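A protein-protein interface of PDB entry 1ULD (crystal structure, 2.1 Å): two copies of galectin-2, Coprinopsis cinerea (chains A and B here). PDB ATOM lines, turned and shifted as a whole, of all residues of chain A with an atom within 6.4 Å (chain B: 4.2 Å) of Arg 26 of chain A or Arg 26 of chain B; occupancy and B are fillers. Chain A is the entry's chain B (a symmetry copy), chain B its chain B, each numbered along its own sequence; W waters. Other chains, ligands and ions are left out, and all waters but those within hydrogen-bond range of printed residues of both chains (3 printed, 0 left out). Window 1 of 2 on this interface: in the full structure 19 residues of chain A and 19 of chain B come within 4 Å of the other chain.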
ATOM      1  N   MET A   1       2.911 -12.153  -8.006  1.00  0.00           N
ATOM      2  CA  MET A   1       2.552 -10.713  -7.961  1.00  0.00           C
ATOM      3  C   MET A   1       2.100 -10.266  -9.346  1.00  0.00           C
ATOM      4  O   MET A   1       2.837 -10.405 -10.323  1.00  0.00           O
ATOM      5  CB  MET A   1       3.757  -9.889  -7.524  1.00  0.00           C
ATOM      6  CG  MET A   1       3.495  -8.401  -7.463  1.00  0.00           C
ATOM      7  SD  MET A   1       2.348  -7.967  -6.153  1.00  0.00           S
ATOM      8  CE  MET A   1       3.436  -8.040  -4.743  1.00  0.00           C
ATOM      9  N   LEU A   2       0.884  -9.732  -9.421  1.00  0.00           N
ATOM     10  CA  LEU A   2       0.318  -9.278 -10.685  1.00  0.00           C
ATOM     11  C   LEU A   2       0.517  -7.795 -10.935  1.00  0.00           C
ATOM     12  O   LEU A   2       0.295  -6.976 -10.045  1.00  0.00           O
ATOM     13  CB  LEU A   2      -1.185  -9.575 -10.724  1.00  0.00           C
ATOM     14  CG  LEU A   2      -1.973  -8.926 -11.870  1.00  0.00           C
ATOM     15  CD1 LEU A   2      -1.612  -9.592 -13.197  1.00  0.00           C
ATOM     16  CD2 LEU A   2      -3.470  -9.045 -11.597  1.00  0.00           C
ATOM     17  N   HIS A   4       0.026  -4.649 -14.171  1.00  0.00           N
ATOM     18  CA  HIS A   4      -0.593  -4.306 -15.446  1.00  0.00           C
ATOM     19  C   HIS A   4       0.378  -3.308 -16.062  1.00  0.00           C
ATOM     20  O   HIS A   4       0.455  -2.154 -15.645  1.00  0.00           O
ATOM     21  CB  HIS A   4      -1.978  -3.685 -15.237  1.00  0.00           C
ATOM     22  CG  HIS A   4      -3.037  -4.694 -14.903  1.00  0.00           C
ATOM     23  ND1 HIS A   4      -3.899  -4.551 -13.837  1.00  0.00           N
ATOM     24  CD2 HIS A   4      -3.354  -5.873 -15.486  1.00  0.00           C
ATOM     25  CE1 HIS A   4      -4.698  -5.601 -13.777  1.00  0.00           C
ATOM     26  NE2 HIS A   4      -4.389  -6.419 -14.765  1.00  0.00           N
ATOM     27  N   ALA A  24       5.820 -13.790 -16.238  1.00  0.00           N
ATOM     28  CA  ALA A  24       4.904 -14.325 -17.242  1.00  0.00           C
ATOM     29  C   ALA A  24       4.109 -13.163 -17.812  1.00  0.00           C
ATOM     30  O   ALA A  24       3.192 -12.657 -17.164  1.00  0.00           O
ATOM     31  CB  ALA A  24       3.958 -15.345 -16.613  1.00  0.00           C
ATOM     32  N   ILE A  25       4.476 -12.729 -19.016  1.00  0.00           N
ATOM     33  CA  ILE A  25       3.791 -11.613 -19.672  1.00  0.00           C
ATOM     34  C   ILE A  25       2.724 -12.162 -20.612  1.00  0.00           C
ATOM     35  O   ILE A  25       3.010 -13.025 -21.447  1.00  0.00           O
ATOM     36  CB  ILE A  25       4.774 -10.755 -20.516  1.00  0.00           C
ATOM     37  CG1 ILE A  25       5.929 -10.262 -19.642  1.00  0.00           C
ATOM     38  CG2 ILE A  25       4.032  -9.580 -21.139  1.00  0.00           C
ATOM     39  CD1 ILE A  25       7.026  -9.562 -20.427  1.00  0.00           C
ATOM     40  N   ARG A  26       1.501 -11.657 -20.486  1.00  0.00           N
ATOM     41  CA  ARG A  26       0.417 -12.121 -21.341  1.00  0.00           C
ATOM     42  C   ARG A  26      -0.383 -10.964 -21.918  1.00  0.00           C
ATOM     43  O   ARG A  26      -0.713 -10.006 -21.211  1.00  0.00           O
ATOM     44  CB  ARG A  26      -0.497 -13.069 -20.557  1.00  0.00           C
ATOM     45  CG  ARG A  26       0.210 -14.349 -20.090  1.00  0.00           C
ATOM     46  CD  ARG A  26      -0.753 -15.338 -19.442  1.00  0.00           C
ATOM     47  NE  ARG A  26      -1.395 -14.803 -18.238  1.00  0.00           N
ATOM     48  CZ  ARG A  26      -2.713 -14.736 -18.063  1.00  0.00           C
ATOM     49  NH1 ARG A  26      -3.528 -15.164 -19.017  1.00  0.00           N
ATOM     50  NH2 ARG A  26      -3.219 -14.256 -16.929  1.00  0.00           N
ATOM     51  N   SER A  27      -0.686 -11.056 -23.209  1.00  0.00           N
ATOM     52  CA  SER A  27      -1.448 -10.018 -23.901  1.00  0.00           C
ATOM     53  C   SER A  27      -2.874 -10.472 -24.168  1.00  0.00           C
ATOM     54  O   SER A  27      -3.109 -11.643 -24.453  1.00  0.00           O
ATOM     55  CB  SER A  27      -0.776  -9.664 -25.236  1.00  0.00           C
ATOM     56  OG  SER A  27      -1.589  -8.782 -25.992  1.00  0.00           O
ATOM     57  N   SER A  28      -3.825  -9.543 -24.078  1.00  0.00           N
ATOM     58  CA  SER A  28      -5.232  -9.865 -24.323  1.00  0.00           C
ATOM     59  C   SER A  28      -5.558  -9.804 -25.808  1.00  0.00           C
ATOM     60  O   SER A  28      -6.709  -9.991 -26.211  1.00  0.00           O
ATOM     61  CB  SER A  28      -6.146  -8.896 -23.573  1.00  0.00           C
ATOM     62  OG  SER A  28      -5.839  -7.550 -23.896  1.00  0.00           O
ATOM     63  N   ASN A  88      -4.120 -14.490 -27.564  1.00  0.00           N
ATOM     64  CA  ASN A  88      -3.485 -14.203 -26.275  1.00  0.00           C
ATOM     65  C   ASN A  88      -2.022 -14.647 -26.285  1.00  0.00           C
ATOM     66  O   ASN A  88      -1.676 -15.673 -25.693  1.00  0.00           O
ATOM     67  CB  ASN A  88      -4.214 -14.943 -25.149  1.00  0.00           C
ATOM     68  CG  ASN A  88      -5.644 -14.455 -24.932  1.00  0.00           C
ATOM     69  OD1 ASN A  88      -6.435 -15.134 -24.275  1.00  0.00           O
ATOM     70  ND2 ASN A  88      -5.977 -13.282 -25.463  1.00  0.00           N
ATOM     71  N   PRO A  89      -1.144 -13.888 -26.968  1.00  0.00           N
ATOM     72  CA  PRO A  89       0.277 -14.252 -27.022  1.00  0.00           C
ATOM     73  C   PRO A  89       0.985 -14.044 -25.684  1.00  0.00           C
ATOM     74  O   PRO A  89       0.559 -13.230 -24.865  1.00  0.00           O
ATOM     75  CB  PRO A  89       0.822 -13.348 -28.127  1.00  0.00           C
ATOM     76  CG  PRO A  89      -0.054 -12.142 -28.039  1.00  0.00           C
ATOM     77  CD  PRO A  89      -1.423 -12.736 -27.843  1.00  0.00           C
ATOM     78  N   SER A  90       2.065 -14.784 -25.463  1.00  0.00           N
ATOM     79  CA  SER A  90       2.795 -14.656 -24.214  1.00  0.00           C
ATOM     80  C   SER A  90       4.311 -14.607 -24.366  1.00  0.00           C
ATOM     81  O   SER A  90       4.886 -15.071 -25.362  1.00  0.00           O
ATOM     82  CB  SER A  90       2.439 -15.814 -23.288  1.00  0.00           C
ATOM     83  OG  SER A  90       2.948 -17.026 -23.800  1.00  0.00           O
ATOM     84  N   ILE A  91       4.942 -14.027 -23.348  1.00  0.00           N
ATOM     85  CA  ILE A  91       6.385 -13.910 -23.265  1.00  0.00           C
ATOM     86  C   ILE A  91       6.720 -14.239 -21.820  1.00  0.00           C
ATOM     87  O   ILE A  91       6.206 -13.609 -20.896  1.00  0.00           O
ATOM     88  CB  ILE A  91       6.893 -12.473 -23.551  1.00  0.00           C
ATOM     89  CG1 ILE A  91       6.496 -12.032 -24.958  1.00  0.00           C
ATOM     90  CG2 ILE A  91       8.410 -12.430 -23.409  1.00  0.00           C
ATOM     91  CD1 ILE A  91       6.858 -10.574 -25.264  1.00  0.00           C
ATOM     92  N   SER A 133      -1.617  -5.937 -26.474  1.00  0.00           N
ATOM     93  CA  SER A 133      -2.576  -5.073 -25.799  1.00  0.00           C
ATOM     94  C   SER A 133      -1.898  -4.150 -24.796  1.00  0.00           C
ATOM     95  O   SER A 133      -0.753  -4.362 -24.398  1.00  0.00           O
ATOM     96  CB  SER A 133      -3.610  -5.925 -25.054  1.00  0.00           C
ATOM     97  OG  SER A 133      -2.977  -6.714 -24.050  1.00  0.00           O
ATOM     98  N   PRO A 135      -2.951  -2.536 -21.130  1.00  0.00           N
ATOM     99  CA  PRO A 135      -1.641  -3.047 -20.716  1.00  0.00           C
ATOM    100  C   PRO A 135      -1.519  -4.530 -21.035  1.00  0.00           C
ATOM    101  O   PRO A 135      -2.409  -5.120 -21.651  1.00  0.00           O
ATOM    102  CB  PRO A 135      -1.663  -2.822 -19.211  1.00  0.00           C
ATOM    103  CG  PRO A 135      -3.085  -3.192 -18.878  1.00  0.00           C
ATOM    104  CD  PRO A 135      -3.883  -2.494 -19.987  1.00  0.00           C
ATOM    105  N   VAL A 136      -0.401  -5.123 -20.636  1.00  0.00           N
ATOM    106  CA  VAL A 136      -0.220  -6.557 -20.781  1.00  0.00           C
ATOM    107  C   VAL A 136      -0.256  -7.044 -19.337  1.00  0.00           C
ATOM    108  O   VAL A 136       0.126  -6.315 -18.417  1.00  0.00           O
ATOM    109  CB  VAL A 136       1.130  -6.954 -21.433  1.00  0.00           C
ATOM    110  CG1 VAL A 136       1.093  -6.644 -22.920  1.00  0.00           C
ATOM    111  CG2 VAL A 136       2.286  -6.229 -20.764  1.00  0.00           C
ATOM    112  N   THR A 137      -0.754  -8.257 -19.138  1.00  0.00           N
ATOM    113  CA  THR A 137      -0.829  -8.831 -17.812  1.00  0.00           C
ATOM    114  C   THR A 137       0.534  -9.430 -17.509  1.00  0.00           C
ATOM    115  O   THR A 137       1.085 -10.167 -18.320  1.00  0.00           O
ATOM    116  CB  THR A 137      -1.953  -9.910 -17.745  1.00  0.00           C
ATOM    117  OG1 THR A 137      -3.222  -9.251 -17.604  1.00  0.00           O
ATOM    118  CG2 THR A 137      -1.734 -10.881 -16.575  1.00  0.00           C
ATOM    119  N   VAL A 138       1.086  -9.088 -16.349  1.00  0.00           N
ATOM    120  CA  VAL A 138       2.391  -9.594 -15.955  1.00  0.00           C
ATOM    121  C   VAL A 138       2.362 -10.209 -14.565  1.00  0.00           C
ATOM    122  O   VAL A 138       2.085  -9.521 -13.576  1.00  0.00           O
ATOM    123  CB  VAL A 138       3.460  -8.481 -15.950  1.00  0.00           C
ATOM    124  CG1 VAL A 138       4.850  -9.107 -15.807  1.00  0.00           C
ATOM    125  CG2 VAL A 138       3.368  -7.641 -17.227  1.00  0.00           C
ATOM    126  N   ASP A 139       2.639 -11.509 -14.501  1.00  0.00           N
ATOM    127  CA  ASP A 139       2.695 -12.217 -13.236  1.00  0.00           C
ATOM    128  C   ASP A 139       4.155 -12.534 -12.954  1.00  0.00           C
ATOM    129  O   ASP A 139       4.801 -13.251 -13.719  1.00  0.00           O
ATOM    130  CB  ASP A 139       1.872 -13.504 -13.299  1.00  0.00           C
ATOM    131  CG  ASP A 139       0.385 -13.244 -13.154  1.00  0.00           C
ATOM    132  OD1 ASP A 139      -0.024 -12.808 -12.057  1.00  0.00           O
ATOM    133  OD2 ASP A 139      -0.363 -13.466 -14.131  1.00  0.00           O
ATOM    134  N   LEU B   2      -7.819 -14.637 -22.176  1.00  0.00           N
ATOM    135  CA  LEU B   2      -7.522 -13.474 -21.350  1.00  0.00           C
ATOM    136  C   LEU B   2      -8.181 -12.201 -21.845  1.00  0.00           C
ATOM    137  O   LEU B   2      -8.145 -11.903 -23.038  1.00  0.00           O
ATOM    138  CB  LEU B   2      -6.009 -13.241 -21.292  1.00  0.00           C
ATOM    139  CG  LEU B   2      -5.551 -11.909 -20.683  1.00  0.00           C
ATOM    140  CD1 LEU B   2      -5.800 -11.909 -19.175  1.00  0.00           C
ATOM    141  CD2 LEU B   2      -4.071 -11.687 -20.984  1.00  0.00           C
ATOM    142  N   ALA B  24     -11.835 -16.093 -13.865  1.00  0.00           N
ATOM    143  CA  ALA B  24     -10.885 -15.759 -12.807  1.00  0.00           C
ATOM    144  C   ALA B  24     -10.529 -14.289 -12.949  1.00  0.00           C
ATOM    145  O   ALA B  24      -9.759 -13.917 -13.835  1.00  0.00           O
ATOM    146  CB  ALA B  24      -9.626 -16.614 -12.928  1.00  0.00           C
ATOM    147  N   ILE B  25     -11.107 -13.454 -12.090  1.00  0.00           N
ATOM    148  CA  ILE B  25     -10.849 -12.013 -12.126  1.00  0.00           C
ATOM    149  C   ILE B  25      -9.747 -11.675 -11.129  1.00  0.00           C
ATOM    150  O   ILE B  25      -9.825 -12.056  -9.956  1.00  0.00           O
ATOM    151  CB  ILE B  25     -12.112 -11.195 -11.735  1.00  0.00           C
ATOM    152  CG1 ILE B  25     -13.286 -11.572 -12.640  1.00  0.00           C
ATOM    153  CG2 ILE B  25     -11.814  -9.705 -11.833  1.00  0.00           C
ATOM    154  CD1 ILE B  25     -14.605 -10.947 -12.214  1.00  0.00           C
ATOM    155  N   ARG B  26      -8.728 -10.954 -11.587  1.00  0.00           N
ATOM    156  CA  ARG B  26      -7.628 -10.584 -10.706  1.00  0.00           C
ATOM    157  C   ARG B  26      -7.267  -9.114 -10.840  1.00  0.00           C
ATOM    158  O   ARG B  26      -7.186  -8.579 -11.952  1.00  0.00           O
ATOM    159  CB  ARG B  26      -6.409 -11.466 -10.994  1.00  0.00           C
ATOM    160  CG  ARG B  26      -6.655 -12.955 -10.711  1.00  0.00           C
ATOM    161  CD  ARG B  26      -5.387 -13.789 -10.866  1.00  0.00           C
ATOM    162  NE  ARG B  26      -4.841 -13.750 -12.226  1.00  0.00           N
ATOM    163  CZ  ARG B  26      -3.595 -13.382 -12.519  1.00  0.00           C
ATOM    164  NH1 ARG B  26      -2.771 -13.015 -11.547  1.00  0.00           N
ATOM    165  NH2 ARG B  26      -3.167 -13.394 -13.779  1.00  0.00           N
ATOM    166  N   SER B  27      -7.058  -8.462  -9.701  1.00  0.00           N
ATOM    167  CA  SER B  27      -6.705  -7.043  -9.673  1.00  0.00           C
ATOM    168  C   SER B  27      -5.236  -6.850  -9.336  1.00  0.00           C
ATOM    169  O   SER B  27      -4.681  -7.594  -8.533  1.00  0.00           O
ATOM    170  CB  SER B  27      -7.560  -6.301  -8.635  1.00  0.00           C
ATOM    171  OG  SER B  27      -7.118  -4.963  -8.481  1.00  0.00           O
ATOM    172  N   PRO B  89      -6.073  -8.786  -5.087  1.00  0.00           N
ATOM    173  CA  PRO B  89      -7.316  -9.487  -4.745  1.00  0.00           C
ATOM    174  C   PRO B  89      -7.941 -10.190  -5.949  1.00  0.00           C
ATOM    175  O   PRO B  89      -7.716  -9.800  -7.094  1.00  0.00           O
ATOM    176  CB  PRO B  89      -8.198  -8.371  -4.187  1.00  0.00           C
ATOM    177  CG  PRO B  89      -7.725  -7.164  -4.928  1.00  0.00           C
ATOM    178  CD  PRO B  89      -6.229  -7.331  -4.918  1.00  0.00           C
ATOM    179  N   SER B  90      -8.724 -11.229  -5.688  1.00  0.00           N
ATOM    180  CA  SER B  90      -9.354 -11.962  -6.773  1.00  0.00           C
ATOM    181  C   SER B  90     -10.821 -12.306  -6.542  1.00  0.00           C
ATOM    182  O   SER B  90     -11.307 -12.369  -5.403  1.00  0.00           O
ATOM    183  CB  SER B  90      -8.589 -13.254  -7.037  1.00  0.00           C
ATOM    184  OG  SER B  90      -8.748 -14.146  -5.954  1.00  0.00           O
ATOM    185  N   VAL B 136      -8.915  -4.970 -14.825  1.00  0.00           N
ATOM    186  CA  VAL B 136      -8.664  -6.124 -13.980  1.00  0.00           C
ATOM    187  C   VAL B 136      -8.364  -7.221 -14.994  1.00  0.00           C
ATOM    188  O   VAL B 136      -8.872  -7.195 -16.119  1.00  0.00           O
ATOM    189  CB  VAL B 136      -9.879  -6.537 -13.108  1.00  0.00           C
ATOM    190  CG1 VAL B 136     -10.060  -5.541 -11.975  1.00  0.00           C
ATOM    191  CG2 VAL B 136     -11.141  -6.625 -13.950  1.00  0.00           C
ATOM    192  N   THR B 137      -7.508  -8.158 -14.611  1.00  0.00           N
ATOM    193  CA  THR B 137      -7.153  -9.257 -15.485  1.00  0.00           C
ATOM    194  C   THR B 137      -8.241 -10.307 -15.341  1.00  0.00           C
ATOM    195  O   THR B 137      -8.608 -10.677 -14.230  1.00  0.00           O
ATOM    196  CB  THR B 137      -5.753  -9.829 -15.105  1.00  0.00           C
ATOM    197  OG1 THR B 137      -4.737  -8.976 -15.655  1.00  0.00           O
ATOM    198  CG2 THR B 137      -5.571 -11.264 -15.623  1.00  0.00           C
ATOM    199  N   ASP B 139      -9.362 -14.121 -16.754  1.00  0.00           N
ATOM    200  CA  ASP B 139      -9.097 -15.338 -17.497  1.00  0.00           C
ATOM    201  C   ASP B 139     -10.365 -16.178 -17.466  1.00  0.00           C
ATOM    202  O   ASP B 139     -10.823 -16.583 -16.398  1.00  0.00           O
ATOM    203  CB  ASP B 139      -7.931 -16.109 -16.878  1.00  0.00           C
ATOM    204  CG  ASP B 139      -6.587 -15.517 -17.253  1.00  0.00           C
ATOM    205  OD1 ASP B 139      -6.240 -15.577 -18.452  1.00  0.00           O
ATOM    206  OD2 ASP B 139      -5.889 -14.991 -16.359  1.00  0.00           O
HETATM  207  O   HOH W   1      -9.072 -10.505 -25.001  1.00  0.00           O
HETATM  208  O   HOH W   2      -4.112 -16.569 -14.588  1.00  0.00           O
HETATM  209  O   HOH W   3      -1.427 -16.163 -14.744  1.00  0.00           O
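The backbone NH of Leu 2 of chain B lies within hydrogen-bond range of the side-chain amide oxygen of Asn 88 of chain A (2.6 Å).
OG1 of Thr 137 of chain A lies within hydrogen-bond range of OG1 of Thr 137 of chain B, at 2.5 Å.
OG1 of Thr 137 of chain B is in hydrogen-bond range of NE2 of His 4 of chain A.
The guanidinium group (NH1) of Arg 26 of chain B is in salt-bridge range of the side-chain carboxylate (OD1) of Asp 139 of chain A.
NH2 of Arg 26 of chain B lies close to NH2 of Arg 26 of chain A (3.3 Å).
The side-chain carboxylate (OD1) of Asp 139 of chain B lies within salt-bridge range of the guanidinium group (NH1) of Arg 26 of chain A (2.8 Å).
N of Ser 27 of chain B is in hydrogen-bond range of O of Pro 89 of chain B, at 3.0 Å.
The backbone NH of Ser 28 of chain A is in hydrogen-bond range of the side-chain hydroxyl of Ser 133 of chain A (3.0 Å).
The backbone carbonyl oxygen (O) of Thr 137 of chain B is in hydrogen-bond range of the backbone NH (N) of Arg 26 of chain B, 2.7 Å away.
The backbone NH of Ala 24 of chain A lies within hydrogen-bond range of the backbone carbonyl oxygen of Asp 139 of chain A (2.8 Å).
The side-chain hydroxyl of Ser 27 of chain A sits at hydrogen-bond distance from the backbone NH of Ser 133 of chain A (2.9 Å).
ND2 of Asn 88 of chain A is in hydrogen-bond range of O of Ser 28 of chain A.
Leu 2 of chain A touches Arg 26 of chain B (CD2 to O, 3.8 Å).
Leu 2 of chain A touches Ser 27 of chain B.
O of Arg 26 of chain A touches CD2 of Leu 2 of chain B (3.8 Å).
CD2 of Leu 2 of chain B touches O of Ser 27 of chain A, at 3.6 Å.
Ser 28 of chain A touches Leu 2 of chain B.
Of chain B, only Leu 2, Arg 26 and Asp 139 come within 4 Å of Arg 26 of chain A.
Of chain A, only Leu 2 (3.8 Å), Arg 26 (3.3 Å) and Asp 139 (2.8 Å) come within 4 Å of Arg 26 of chain B.
Of the printed residues of chain A, Ser 27 of chain B touches Leu 2.
Of the printed residues of chain A, Asp 139 of chain B touches Arg 26.
Of the printed residues of chain B, Ser 28 of chain A touches Leu 2.
Of the printed residues of chain B, His 4 of chain A touches Thr 137.
Val 136 of chain A touches none of the printed residues of chain B.
Val 136 of chain B touches none of the printed residues of chain A.
The nearest residue of chain A that does not touch Arg 26 of chain B is Thr 137 of chain A (4.02 Å).
Of the 18 printed residues of chain A, 8 touch a printed residue of chain B.
Hydrophobic or aromatic side chains of chain B within 4 Å of the printed part of chain A: Leu 2.
Among the printed residues, Asp or Glu carboxylates within 4 Å of a Lys or Arg side-chain nitrogen of the other chain: Arg 26 of chain A with Asp 139 of chain B (2.8 Å) and Asp 139 of chain A with Arg 26 of chain B (2.8 Å).
Leu 2 of chain A touches Arg 26 of chain B, and with the chains exchanged Arg 26 of chain A touches Leu 2 of chain B.
Leu 2 of chain A touches Ser 27 of chain B, and with the chains exchanged Ser 27 of chain A touches Leu 2 of chain B.
Arg 26 of chain A touches its own counterpart, Arg 26 of chain B.
Arg 26 of chain A touches Asp 139 of chain B, and with the chains exchanged Asp 139 of chain A touches Arg 26 of chain B.
10 positions are printed for both chains.
Water W1 bridges O of Leu 2 of chain B and O of Ser 28 of chain A.
Water W3 lies within hydrogen-bond range of OD2 of Asp 139 of chain A (3.0 Å), NH2 of Arg 26 of chain A (3.4 Å) and NH2 of Arg 26 of chain B (3.4 Å).
Water W2 lies within hydrogen-bond range of OD2 of Asp 139 of chain B (3.0 Å), NH2 of Arg 26 of chain B (3.4 Å) and NH2 of Arg 26 of chain A (3.4 Å).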
